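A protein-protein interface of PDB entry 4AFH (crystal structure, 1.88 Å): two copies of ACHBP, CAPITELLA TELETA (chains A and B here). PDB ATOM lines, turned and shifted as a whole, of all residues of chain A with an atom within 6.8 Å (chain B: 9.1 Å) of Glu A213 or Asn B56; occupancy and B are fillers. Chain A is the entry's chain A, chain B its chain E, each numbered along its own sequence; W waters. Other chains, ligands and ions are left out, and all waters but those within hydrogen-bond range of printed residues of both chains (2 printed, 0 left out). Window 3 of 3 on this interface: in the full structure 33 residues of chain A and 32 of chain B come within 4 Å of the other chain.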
ATOM      1  N   LEU A  45      -9.201 -20.469  21.940  1.00  0.00           N
ATOM      2  CA  LEU A  45      -8.993 -21.584  21.005  1.00  0.00           C
ATOM      3  C   LEU A  45     -10.247 -22.451  20.927  1.00  0.00           C
ATOM      4  O   LEU A  45     -10.725 -22.941  21.951  1.00  0.00           O
ATOM      5  CB  LEU A  45      -7.822 -22.455  21.485  1.00  0.00           C
ATOM      6  CG  LEU A  45      -7.424 -23.670  20.617  1.00  0.00           C
ATOM      7  CD1 LEU A  45      -6.717 -23.247  19.324  1.00  0.00           C
ATOM      8  CD2 LEU A  45      -6.535 -24.614  21.413  1.00  0.00           C
ATOM      9  N   ILE A  48      -7.681 -27.742  18.619  1.00  0.00           N
ATOM     10  CA  ILE A  48      -6.421 -27.995  17.960  1.00  0.00           C
ATOM     11  C   ILE A  48      -6.370 -29.501  17.767  1.00  0.00           C
ATOM     12  O   ILE A  48      -6.384 -30.281  18.718  1.00  0.00           O
ATOM     13  CB  ILE A  48      -5.213 -27.409  18.719  1.00  0.00           C
ATOM     14  CG1 ILE A  48      -3.936 -27.568  17.890  1.00  0.00           C
ATOM     15  CG2 ILE A  48      -5.056 -28.017  20.105  1.00  0.00           C
ATOM     16  CD1 ILE A  48      -3.018 -26.368  17.996  1.00  0.00           C
ATOM     17  N   ASP A 142       4.771 -30.607  23.886  1.00  0.00           N
ATOM     18  CA  ASP A 142       3.683 -29.971  24.636  1.00  0.00           C
ATOM     19  C   ASP A 142       3.536 -28.472  24.347  1.00  0.00           C
ATOM     20  O   ASP A 142       2.950 -27.729  25.135  1.00  0.00           O
ATOM     21  CB  ASP A 142       3.793 -30.245  26.146  1.00  0.00           C
ATOM     22  CG  ASP A 142       3.767 -31.734  26.471  1.00  0.00           C
ATOM     23  OD1 ASP A 142       3.394 -32.536  25.588  1.00  0.00           O
ATOM     24  OD2 ASP A 142       4.118 -32.108  27.613  1.00  0.00           O
ATOM     25  N   ASP A 144       2.170 -25.893  21.160  1.00  0.00           N
ATOM     26  CA  ASP A 144       1.559 -25.771  19.843  1.00  0.00           C
ATOM     27  C   ASP A 144       1.936 -24.419  19.279  1.00  0.00           C
ATOM     28  O   ASP A 144       1.547 -23.394  19.833  1.00  0.00           O
ATOM     29  CB  ASP A 144       0.037 -25.888  19.936  1.00  0.00           C
ATOM     30  CG  ASP A 144      -0.418 -27.205  20.542  1.00  0.00           C
ATOM     31  OD1 ASP A 144       0.058 -28.262  20.093  1.00  0.00           O
ATOM     32  OD2 ASP A 144      -1.239 -27.183  21.480  1.00  0.00           O
ATOM     33  N   ASP A 178      -9.372 -17.334  27.533  1.00  0.00           N
ATOM     34  CA  ASP A 178      -9.141 -18.769  27.538  1.00  0.00           C
ATOM     35  C   ASP A 178      -8.212 -19.064  28.703  1.00  0.00           C
ATOM     36  O   ASP A 178      -7.667 -18.131  29.297  1.00  0.00           O
ATOM     37  CB  ASP A 178      -8.523 -19.179  26.205  1.00  0.00           C
ATOM     38  CG  ASP A 178      -8.787 -20.631  25.859  1.00  0.00           C
ATOM     39  OD1 ASP A 178      -8.682 -21.502  26.754  1.00  0.00           O
ATOM     40  OD2 ASP A 178      -9.084 -20.905  24.681  1.00  0.00           O
ATOM     41  N   SER A 179      -8.046 -20.327  29.053  1.00  0.00           N
ATOM     42  CA  SER A 179      -7.152 -20.687  30.157  1.00  0.00           C
ATOM     43  C   SER A 179      -5.748 -21.045  29.672  1.00  0.00           C
ATOM     44  O   SER A 179      -4.849 -21.264  30.474  1.00  0.00           O
ATOM     45  CB  SER A 179      -7.723 -21.879  30.918  1.00  0.00           C
ATOM     46  OG  SER A 179      -7.943 -22.953  30.018  1.00  0.00           O
ATOM     47  N   LEU A 180      -5.564 -21.136  28.362  1.00  0.00           N
ATOM     48  CA  LEU A 180      -4.292 -21.623  27.813  1.00  0.00           C
ATOM     49  C   LEU A 180      -3.165 -20.633  28.057  1.00  0.00           C
ATOM     50  O   LEU A 180      -3.337 -19.425  27.901  1.00  0.00           O
ATOM     51  CB  LEU A 180      -4.403 -21.897  26.310  1.00  0.00           C
ATOM     52  CG  LEU A 180      -5.362 -22.983  25.819  1.00  0.00           C
ATOM     53  CD1 LEU A 180      -5.493 -22.900  24.317  1.00  0.00           C
ATOM     54  CD2 LEU A 180      -4.868 -24.352  26.224  1.00  0.00           C
ATOM     55  N   LEU A 210       1.201 -21.782  22.187  1.00  0.00           N
ATOM     56  CA  LEU A 210       0.391 -22.044  23.353  1.00  0.00           C
ATOM     57  C   LEU A 210       0.821 -23.349  23.980  1.00  0.00           C
ATOM     58  O   LEU A 210       1.291 -24.270  23.302  1.00  0.00           O
ATOM     59  CB  LEU A 210      -1.084 -22.186  22.951  1.00  0.00           C
ATOM     60  CG  LEU A 210      -1.709 -21.071  22.121  1.00  0.00           C
ATOM     61  CD1 LEU A 210      -3.029 -21.558  21.539  1.00  0.00           C
ATOM     62  CD2 LEU A 210      -1.953 -19.869  22.980  1.00  0.00           C
ATOM     63  N   ARG A 211       0.610 -23.457  25.278  1.00  0.00           N
ATOM     64  CA  ARG A 211       0.919 -24.704  25.952  1.00  0.00           C
ATOM     65  C   ARG A 211      -0.167 -25.725  25.605  1.00  0.00           C
ATOM     66  O   ARG A 211      -1.341 -25.411  25.653  1.00  0.00           O
ATOM     67  CB  ARG A 211       0.969 -24.453  27.455  1.00  0.00           C
ATOM     68  CG  ARG A 211       0.899 -25.706  28.269  1.00  0.00           C
ATOM     69  CD  ARG A 211       2.239 -26.361  28.280  1.00  0.00           C
ATOM     70  NE  ARG A 211       3.213 -25.507  28.938  1.00  0.00           N
ATOM     71  CZ  ARG A 211       4.513 -25.524  28.657  1.00  0.00           C
ATOM     72  NH1 ARG A 211       4.986 -26.346  27.730  1.00  0.00           N
ATOM     73  NH2 ARG A 211       5.331 -24.721  29.309  1.00  0.00           N
ATOM     74  N   SER A 212       0.226 -26.946  25.241  1.00  0.00           N
ATOM     75  CA  SER A 212      -0.750 -27.963  24.869  1.00  0.00           C
ATOM     76  C   SER A 212      -1.533 -28.406  26.090  1.00  0.00           C
ATOM     77  O   SER A 212      -1.000 -28.413  27.192  1.00  0.00           O
ATOM     78  CB  SER A 212      -0.051 -29.177  24.261  1.00  0.00           C
ATOM     79  OG  SER A 212      -1.001 -30.211  24.043  1.00  0.00           O
ATOM     80  N   GLU A 213      -2.789 -28.791  25.891  1.00  0.00           N
ATOM     81  CA  GLU A 213      -3.640 -29.261  26.980  1.00  0.00           C
ATOM     82  C   GLU A 213      -3.513 -30.755  27.238  1.00  0.00           C
ATOM     83  O   GLU A 213      -3.420 -31.545  26.300  1.00  0.00           O
ATOM     84  CB  GLU A 213      -5.093 -28.924  26.668  1.00  0.00           C
ATOM     85  CG  GLU A 213      -5.441 -27.533  27.052  1.00  0.00           C
ATOM     86  CD  GLU A 213      -6.872 -27.168  26.712  1.00  0.00           C
ATOM     87  OE1 GLU A 213      -7.353 -27.532  25.619  1.00  0.00           O
ATOM     88  OE2 GLU A 213      -7.517 -26.521  27.546  1.00  0.00           O
ATOM     89  N   ILE B  48     -21.943 -30.990  24.974  1.00  0.00           N
ATOM     90  CA  ILE B  48     -20.843 -30.349  25.660  1.00  0.00           C
ATOM     91  C   ILE B  48     -19.642 -31.260  25.425  1.00  0.00           C
ATOM     92  O   ILE B  48     -19.637 -32.424  25.829  1.00  0.00           O
ATOM     93  CB  ILE B  48     -21.152 -30.076  27.158  1.00  0.00           C
ATOM     94  CG1 ILE B  48     -20.003 -29.306  27.817  1.00  0.00           C
ATOM     95  CG2 ILE B  48     -21.477 -31.371  27.907  1.00  0.00           C
ATOM     96  CD1 ILE B  48     -20.457 -28.185  28.722  1.00  0.00           C
ATOM     97  N   GLU B  49     -18.651 -30.754  24.703  1.00  0.00           N
ATOM     98  CA  GLU B  49     -17.558 -31.611  24.243  1.00  0.00           C
ATOM     99  C   GLU B  49     -16.214 -31.137  24.777  1.00  0.00           C
ATOM    100  O   GLU B  49     -15.818 -29.989  24.553  1.00  0.00           O
ATOM    101  CB  GLU B  49     -17.524 -31.676  22.713  1.00  0.00           C
ATOM    102  CG  GLU B  49     -18.762 -32.327  22.076  1.00  0.00           C
ATOM    103  CD  GLU B  49     -18.879 -33.827  22.343  1.00  0.00           C
ATOM    104  OE1 GLU B  49     -17.861 -34.466  22.699  1.00  0.00           O
ATOM    105  OE2 GLU B  49     -19.998 -34.370  22.190  1.00  0.00           O
ATOM    106  N   GLN B  50     -15.517 -32.033  25.469  1.00  0.00           N
ATOM    107  CA  GLN B  50     -14.235 -31.706  26.063  1.00  0.00           C
ATOM    108  C   GLN B  50     -13.305 -31.191  24.978  1.00  0.00           C
ATOM    109  O   GLN B  50     -13.247 -31.751  23.879  1.00  0.00           O
ATOM    110  CB  GLN B  50     -13.614 -32.950  26.732  1.00  0.00           C
ATOM    111  CG  GLN B  50     -12.325 -32.653  27.484  1.00  0.00           C
ATOM    112  CD  GLN B  50     -11.694 -33.884  28.123  1.00  0.00           C
ATOM    113  OE1 GLN B  50     -11.951 -35.023  27.713  1.00  0.00           O
ATOM    114  NE2 GLN B  50     -10.848 -33.656  29.114  1.00  0.00           N
ATOM    115  N   ARG B  51     -12.593 -30.109  25.262  1.00  0.00           N
ATOM    116  CA  ARG B  51     -11.553 -29.685  24.331  1.00  0.00           C
ATOM    117  C   ARG B  51     -10.231 -30.361  24.689  1.00  0.00           C
ATOM    118  O   ARG B  51      -9.734 -30.209  25.798  1.00  0.00           O
ATOM    119  CB  ARG B  51     -11.388 -28.168  24.333  1.00  0.00           C
ATOM    120  CG  ARG B  51     -10.280 -27.688  23.383  1.00  0.00           C
ATOM    121  CD  ARG B  51     -10.119 -26.179  23.480  1.00  0.00           C
ATOM    122  NE  ARG B  51      -9.437 -25.820  24.722  1.00  0.00           N
ATOM    123  CZ  ARG B  51      -9.339 -24.588  25.193  1.00  0.00           C
ATOM    124  NH1 ARG B  51      -9.897 -23.576  24.540  1.00  0.00           N
ATOM    125  NH2 ARG B  51      -8.689 -24.369  26.331  1.00  0.00           N
ATOM    126  N   GLY B  52      -9.662 -31.105  23.748  1.00  0.00           N
ATOM    127  CA  GLY B  52      -8.405 -31.785  24.010  1.00  0.00           C
ATOM    128  C   GLY B  52      -8.520 -32.666  25.241  1.00  0.00           C
ATOM    129  O   GLY B  52      -9.530 -33.334  25.440  1.00  0.00           O
ATOM    130  N   MET B  53      -7.499 -32.649  26.088  1.00  0.00           N
ATOM    131  CA  MET B  53      -7.545 -33.431  27.311  1.00  0.00           C
ATOM    132  C   MET B  53      -7.527 -32.519  28.529  1.00  0.00           C
ATOM    133  O   MET B  53      -7.196 -32.948  29.633  1.00  0.00           O
ATOM    134  CB  MET B  53      -6.398 -34.447  27.340  1.00  0.00           C
ATOM    135  CG  MET B  53      -6.410 -35.405  26.150  1.00  0.00           C
ATOM    136  SD  MET B  53      -5.124 -36.686  26.189  1.00  0.00           S
ATOM    137  CE  MET B  53      -3.650 -35.712  25.899  1.00  0.00           C
ATOM    138  N   GLY B  54      -7.916 -31.259  28.317  1.00  0.00           N
ATOM    139  CA  GLY B  54      -7.943 -30.256  29.369  1.00  0.00           C
ATOM    140  C   GLY B  54      -9.290 -30.123  30.058  1.00  0.00           C
ATOM    141  O   GLY B  54     -10.190 -30.927  29.837  1.00  0.00           O
ATOM    142  N   PHE B  55      -9.438 -29.097  30.888  1.00  0.00           N
ATOM    143  CA  PHE B  55     -10.645 -28.976  31.691  1.00  0.00           C
ATOM    144  C   PHE B  55     -11.661 -28.037  31.071  1.00  0.00           C
ATOM    145  O   PHE B  55     -12.554 -27.552  31.763  1.00  0.00           O
ATOM    146  CB  PHE B  55     -10.316 -28.551  33.127  1.00  0.00           C
ATOM    147  CG  PHE B  55      -9.450 -29.541  33.865  1.00  0.00           C
ATOM    148  CD1 PHE B  55      -9.972 -30.747  34.317  1.00  0.00           C
ATOM    149  CD2 PHE B  55      -8.109 -29.272  34.092  1.00  0.00           C
ATOM    150  CE1 PHE B  55      -9.169 -31.664  34.988  1.00  0.00           C
ATOM    151  CE2 PHE B  55      -7.304 -30.182  34.762  1.00  0.00           C
ATOM    152  CZ  PHE B  55      -7.835 -31.379  35.207  1.00  0.00           C
ATOM    153  N   ASN B  56     -11.515 -27.765  29.775  1.00  0.00           N
ATOM    154  CA  ASN B  56     -12.481 -26.928  29.078  1.00  0.00           C
ATOM    155  C   ASN B  56     -13.288 -27.749  28.067  1.00  0.00           C
ATOM    156  O   ASN B  56     -12.908 -28.853  27.698  1.00  0.00           O
ATOM    157  CB  ASN B  56     -11.825 -25.712  28.399  1.00  0.00           C
ATOM    158  CG  ASN B  56     -11.152 -24.765  29.400  1.00  0.00           C
ATOM    159  OD1 ASN B  56      -9.939 -24.573  29.360  1.00  0.00           O
ATOM    160  ND2 ASN B  56     -11.943 -24.160  30.279  1.00  0.00           N
ATOM    161  N   SER B  57     -14.420 -27.208  27.653  1.00  0.00           N
ATOM    162  CA  SER B  57     -15.281 -27.906  26.720  1.00  0.00           C
ATOM    163  C   SER B  57     -16.018 -26.870  25.892  1.00  0.00           C
ATOM    164  O   SER B  57     -16.150 -25.707  26.307  1.00  0.00           O
ATOM    165  CB  SER B  57     -16.287 -28.748  27.489  1.00  0.00           C
ATOM    166  OG  SER B  57     -17.045 -27.895  28.333  1.00  0.00           O
ATOM    167  N   ILE B  58     -16.478 -27.283  24.724  1.00  0.00           N
ATOM    168  CA  ILE B  58     -17.355 -26.448  23.919  1.00  0.00           C
ATOM    169  C   ILE B  58     -18.790 -26.857  24.242  1.00  0.00           C
ATOM    170  O   ILE B  58     -19.176 -28.023  24.057  1.00  0.00           O
ATOM    171  CB  ILE B  58     -17.158 -26.669  22.408  1.00  0.00           C
ATOM    172  CG1 ILE B  58     -15.681 -26.542  21.999  1.00  0.00           C
ATOM    173  CG2 ILE B  58     -18.051 -25.717  21.639  1.00  0.00           C
ATOM    174  CD1 ILE B  58     -15.013 -25.269  22.436  1.00  0.00           C
ATOM    175  N   GLY B  59     -19.571 -25.901  24.726  1.00  0.00           N
ATOM    176  CA  GLY B  59     -20.962 -26.154  25.055  1.00  0.00           C
ATOM    177  C   GLY B  59     -21.856 -25.553  23.989  1.00  0.00           C
ATOM    178  O   GLY B  59     -21.757 -24.369  23.688  1.00  0.00           O
ATOM    179  N   VAL B 135     -20.320 -21.714  23.293  1.00  0.00           N
ATOM    180  CA  VAL B 135     -19.364 -21.031  24.192  1.00  0.00           C
ATOM    181  C   VAL B 135     -18.348 -22.024  24.773  1.00  0.00           C
ATOM    182  O   VAL B 135     -18.524 -23.238  24.662  1.00  0.00           O
ATOM    183  CB  VAL B 135     -20.096 -20.283  25.355  1.00  0.00           C
ATOM    184  CG1 VAL B 135     -21.005 -19.151  24.794  1.00  0.00           C
ATOM    185  CG2 VAL B 135     -20.921 -21.252  26.224  1.00  0.00           C
ATOM    186  N   LEU B 136     -17.282 -21.502  25.371  1.00  0.00           N
ATOM    187  CA  LEU B 136     -16.223 -22.328  25.945  1.00  0.00           C
ATOM    188  C   LEU B 136     -16.535 -22.437  27.422  1.00  0.00           C
ATOM    189  O   LEU B 136     -16.636 -21.413  28.089  1.00  0.00           O
ATOM    190  CB  LEU B 136     -14.867 -21.638  25.756  1.00  0.00           C
ATOM    191  CG  LEU B 136     -13.602 -22.374  26.198  1.00  0.00           C
ATOM    192  CD1 LEU B 136     -13.335 -23.636  25.334  1.00  0.00           C
ATOM    193  CD2 LEU B 136     -12.426 -21.417  26.142  1.00  0.00           C
ATOM    194  N   CYS B 137     -16.719 -23.660  27.926  1.00  0.00           N
ATOM    195  CA  CYS B 137     -17.106 -23.872  29.318  1.00  0.00           C
ATOM    196  C   CYS B 137     -15.934 -24.446  30.075  1.00  0.00           C
ATOM    197  O   CYS B 137     -14.953 -24.875  29.477  1.00  0.00           O
ATOM    198  CB  CYS B 137     -18.289 -24.847  29.410  1.00  0.00           C
ATOM    199  SG  CYS B 137     -19.752 -24.314  28.456  1.00  0.00           S
ATOM    200  N   VAL B 138     -16.039 -24.433  31.400  1.00  0.00           N
ATOM    201  CA  VAL B 138     -15.081 -25.120  32.250  1.00  0.00           C
ATOM    202  C   VAL B 138     -15.786 -26.358  32.780  1.00  0.00           C
ATOM    203  O   VAL B 138     -16.894 -26.265  33.305  1.00  0.00           O
ATOM    204  CB  VAL B 138     -14.633 -24.235  33.430  1.00  0.00           C
ATOM    205  CG1 VAL B 138     -13.624 -24.981  34.300  1.00  0.00           C
ATOM    206  CG2 VAL B 138     -14.040 -22.933  32.926  1.00  0.00           C
ATOM    207  N   SER B 139     -15.156 -27.515  32.615  1.00  0.00           N
ATOM    208  CA  SER B 139     -15.753 -28.783  33.008  1.00  0.00           C
ATOM    209  C   SER B 139     -14.811 -29.441  33.998  1.00  0.00           C
ATOM    210  O   SER B 139     -13.773 -29.986  33.619  1.00  0.00           O
ATOM    211  CB  SER B 139     -15.974 -29.693  31.795  1.00  0.00           C
ATOM    212  OG  SER B 139     -16.986 -29.198  30.923  1.00  0.00           O
ATOM    213  N   GLN B 140     -15.174 -29.371  35.266  1.00  0.00           N
ATOM    214  CA  GLN B 140     -14.307 -29.837  36.333  1.00  0.00           C
ATOM    215  C   GLN B 140     -15.158 -30.214  37.546  1.00  0.00           C
ATOM    216  O   GLN B 140     -16.153 -29.548  37.843  1.00  0.00           O
ATOM    217  CB  GLN B 140     -13.312 -28.732  36.689  1.00  0.00           C
ATOM    218  CG  GLN B 140     -11.971 -29.235  37.180  1.00  0.00           C
ATOM    219  CD  GLN B 140     -10.925 -28.142  37.202  1.00  0.00           C
ATOM    220  OE1 GLN B 140     -11.248 -26.954  37.100  1.00  0.00           O
ATOM    221  NE2 GLN B 140      -9.661 -28.537  37.325  1.00  0.00           N
ATOM    222  N   VAL B 143     -18.968 -30.604  37.252  1.00  0.00           N
ATOM    223  CA  VAL B 143     -19.738 -29.374  37.029  1.00  0.00           C
ATOM    224  C   VAL B 143     -19.279 -28.732  35.716  1.00  0.00           C
ATOM    225  O   VAL B 143     -18.082 -28.555  35.485  1.00  0.00           O
ATOM    226  CB  VAL B 143     -19.559 -28.360  38.206  1.00  0.00           C
ATOM    227  CG1 VAL B 143     -20.358 -27.076  37.965  1.00  0.00           C
ATOM    228  CG2 VAL B 143     -19.975 -28.993  39.542  1.00  0.00           C
ATOM    229  N   ASP B 144     -20.233 -28.409  34.853  1.00  0.00           N
ATOM    230  CA  ASP B 144     -19.949 -27.661  33.638  1.00  0.00           C
ATOM    231  C   ASP B 144     -20.357 -26.219  33.835  1.00  0.00           C
ATOM    232  O   ASP B 144     -21.545 -25.926  33.967  1.00  0.00           O
ATOM    233  CB  ASP B 144     -20.736 -28.247  32.459  1.00  0.00           C
ATOM    234  CG  ASP B 144     -20.359 -29.696  32.161  1.00  0.00           C
ATOM    235  OD1 ASP B 144     -19.159 -30.000  32.123  1.00  0.00           O
ATOM    236  OD2 ASP B 144     -21.271 -30.525  31.976  1.00  0.00           O
ATOM    237  N   SER B 145     -19.383 -25.311  33.843  1.00  0.00           N
ATOM    238  CA  SER B 145     -19.659 -23.889  34.032  1.00  0.00           C
ATOM    239  C   SER B 145     -19.487 -23.082  32.749  1.00  0.00           C
ATOM    240  O   SER B 145     -18.418 -23.065  32.159  1.00  0.00           O
ATOM    241  CB  SER B 145     -18.728 -23.298  35.101  1.00  0.00           C
ATOM    242  OG  SER B 145     -18.944 -23.902  36.352  1.00  0.00           O
ATOM    243  N   CYS B 146     -20.526 -22.373  32.356  1.00  0.00           N
ATOM    244  CA  CYS B 146     -20.531 -21.681  31.076  1.00  0.00           C
ATOM    245  C   CYS B 146     -20.983 -20.244  31.297  1.00  0.00           C
ATOM    246  O   CYS B 146     -21.843 -19.984  32.132  1.00  0.00           O
ATOM    247  CB  CYS B 146     -21.503 -22.371  30.131  1.00  0.00           C
ATOM    248  SG  CYS B 146     -21.193 -24.136  29.909  1.00  0.00           S
ATOM    249  N   HIS B 147     -20.401 -19.305  30.574  1.00  0.00           N
ATOM    250  CA  HIS B 147     -20.892 -17.929  30.651  1.00  0.00           C
ATOM    251  C   HIS B 147     -21.329 -17.450  29.281  1.00  0.00           C
ATOM    252  O   HIS B 147     -20.896 -18.012  28.268  1.00  0.00           O
ATOM    253  CB  HIS B 147     -19.849 -17.001  31.263  1.00  0.00           C
ATOM    254  CG  HIS B 147     -18.602 -16.839  30.450  1.00  0.00           C
ATOM    255  ND1 HIS B 147     -17.536 -17.714  30.530  1.00  0.00           N
ATOM    256  CD2 HIS B 147     -18.219 -15.859  29.594  1.00  0.00           C
ATOM    257  CE1 HIS B 147     -16.560 -17.295  29.741  1.00  0.00           C
ATOM    258  NE2 HIS B 147     -16.945 -16.170  29.164  1.00  0.00           N
HETATM  259  O   HOH W   1      -7.143 -27.008  30.174  1.00  0.00           O
HETATM  260  O   HOH W   2      -9.740 -28.162  27.678  1.00  0.00           O
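The guanidinium group (NH1) of Arg B51 sits at hydrogen-bond distance from the backbone carbonyl oxygen (O) of Leu A45.
The side-chain carboxylate (OD2) of Asp A178 is in salt-bridge range of the guanidinium group (NH1) of Arg B51 (2.8 Å).
The side-chain hydroxyl of Ser A179 sits at hydrogen-bond distance from the side-chain amide oxygen of Asn B56, 2.7 Å away.
The side-chain carboxylate of Glu A213 is in salt-bridge range of the guanidinium group of Arg B51 (2.7 Å).
Of the printed residues of chain B, Leu A45 touches Arg B51 (2.8 Å).
Of the printed residues of chain B, Asp A178 touches Arg B51 and Leu B136.
Printed residues of chain B within 4 Å of Leu A180: Arg B51 (3.6 Å).
No residue of chain B comes within 4 Å of Ser A212.
Printed residues of chain B within 4 Å of Glu A213: Arg B51 (2.7 Å) and Asn B56 (3.6 Å).
Printed residues of chain A within 4 Å of Arg B51: Leu A45 (2.8 Å), Asp A178 (2.8 Å), Leu A180 (3.6 Å) and Glu A213 (2.7 Å).
Asn B56 touches two residues of chain A.
Printed residues of chain A within 4 Å of Leu B136: Asp A178.
The nearest residue of chain A that does not touch Asn B56 is Asp A178 (4.2 Å).
Of the 11 printed residues of chain A, 5 touch a printed residue of chain B.
Of the 23 printed residues of chain B, 3 touch a printed residue of chain A.
Hydrophobic or aromatic side chains of chain B that line the printed part of chain A: Leu B136.
2 positions are printed for both chains.
Of the 7 pairs that touch across the chains among the printed residues, none has its exchanged pair printed and touching as well.
The side-chain carboxylate (OD2) of Asp A178 lies within hydrogen-bond range of the backbone NH (N) of Leu A45 (2.8 Å).
The backbone NH of Arg B51 sits at hydrogen-bond distance from the backbone carbonyl oxygen of Asn B56 (2.8 Å).
ND2 of Asn B56 sits at hydrogen-bond distance from O of Cys B137 (3.2 Å).
SG of Cys B137 is disulfide-bonded to SG of Cys B146 (2.1 Å).
Water W1 bridges OE2 of Glu A213 and N of Phe B55.
Water W2 lies within hydrogen-bond range of the side-chain carboxylate (OE2) of Glu A213 (2.8 Å), the backbone NH (N) of Asn B56 (2.8 Å), the backbone carbonyl oxygen (O) of Arg B51 (2.8 Å) and the backbone NH (N) of Phe B55 (3.4 Å).
OD2 of Asp A178 touches CD2 of Leu B136, at 3.7 Å.
CG of Leu A180 touches NH2 of Arg B51 (3.6 Å).
Glu A213 touches Asn B56 (OE2 to OD1, 3.6 Å).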
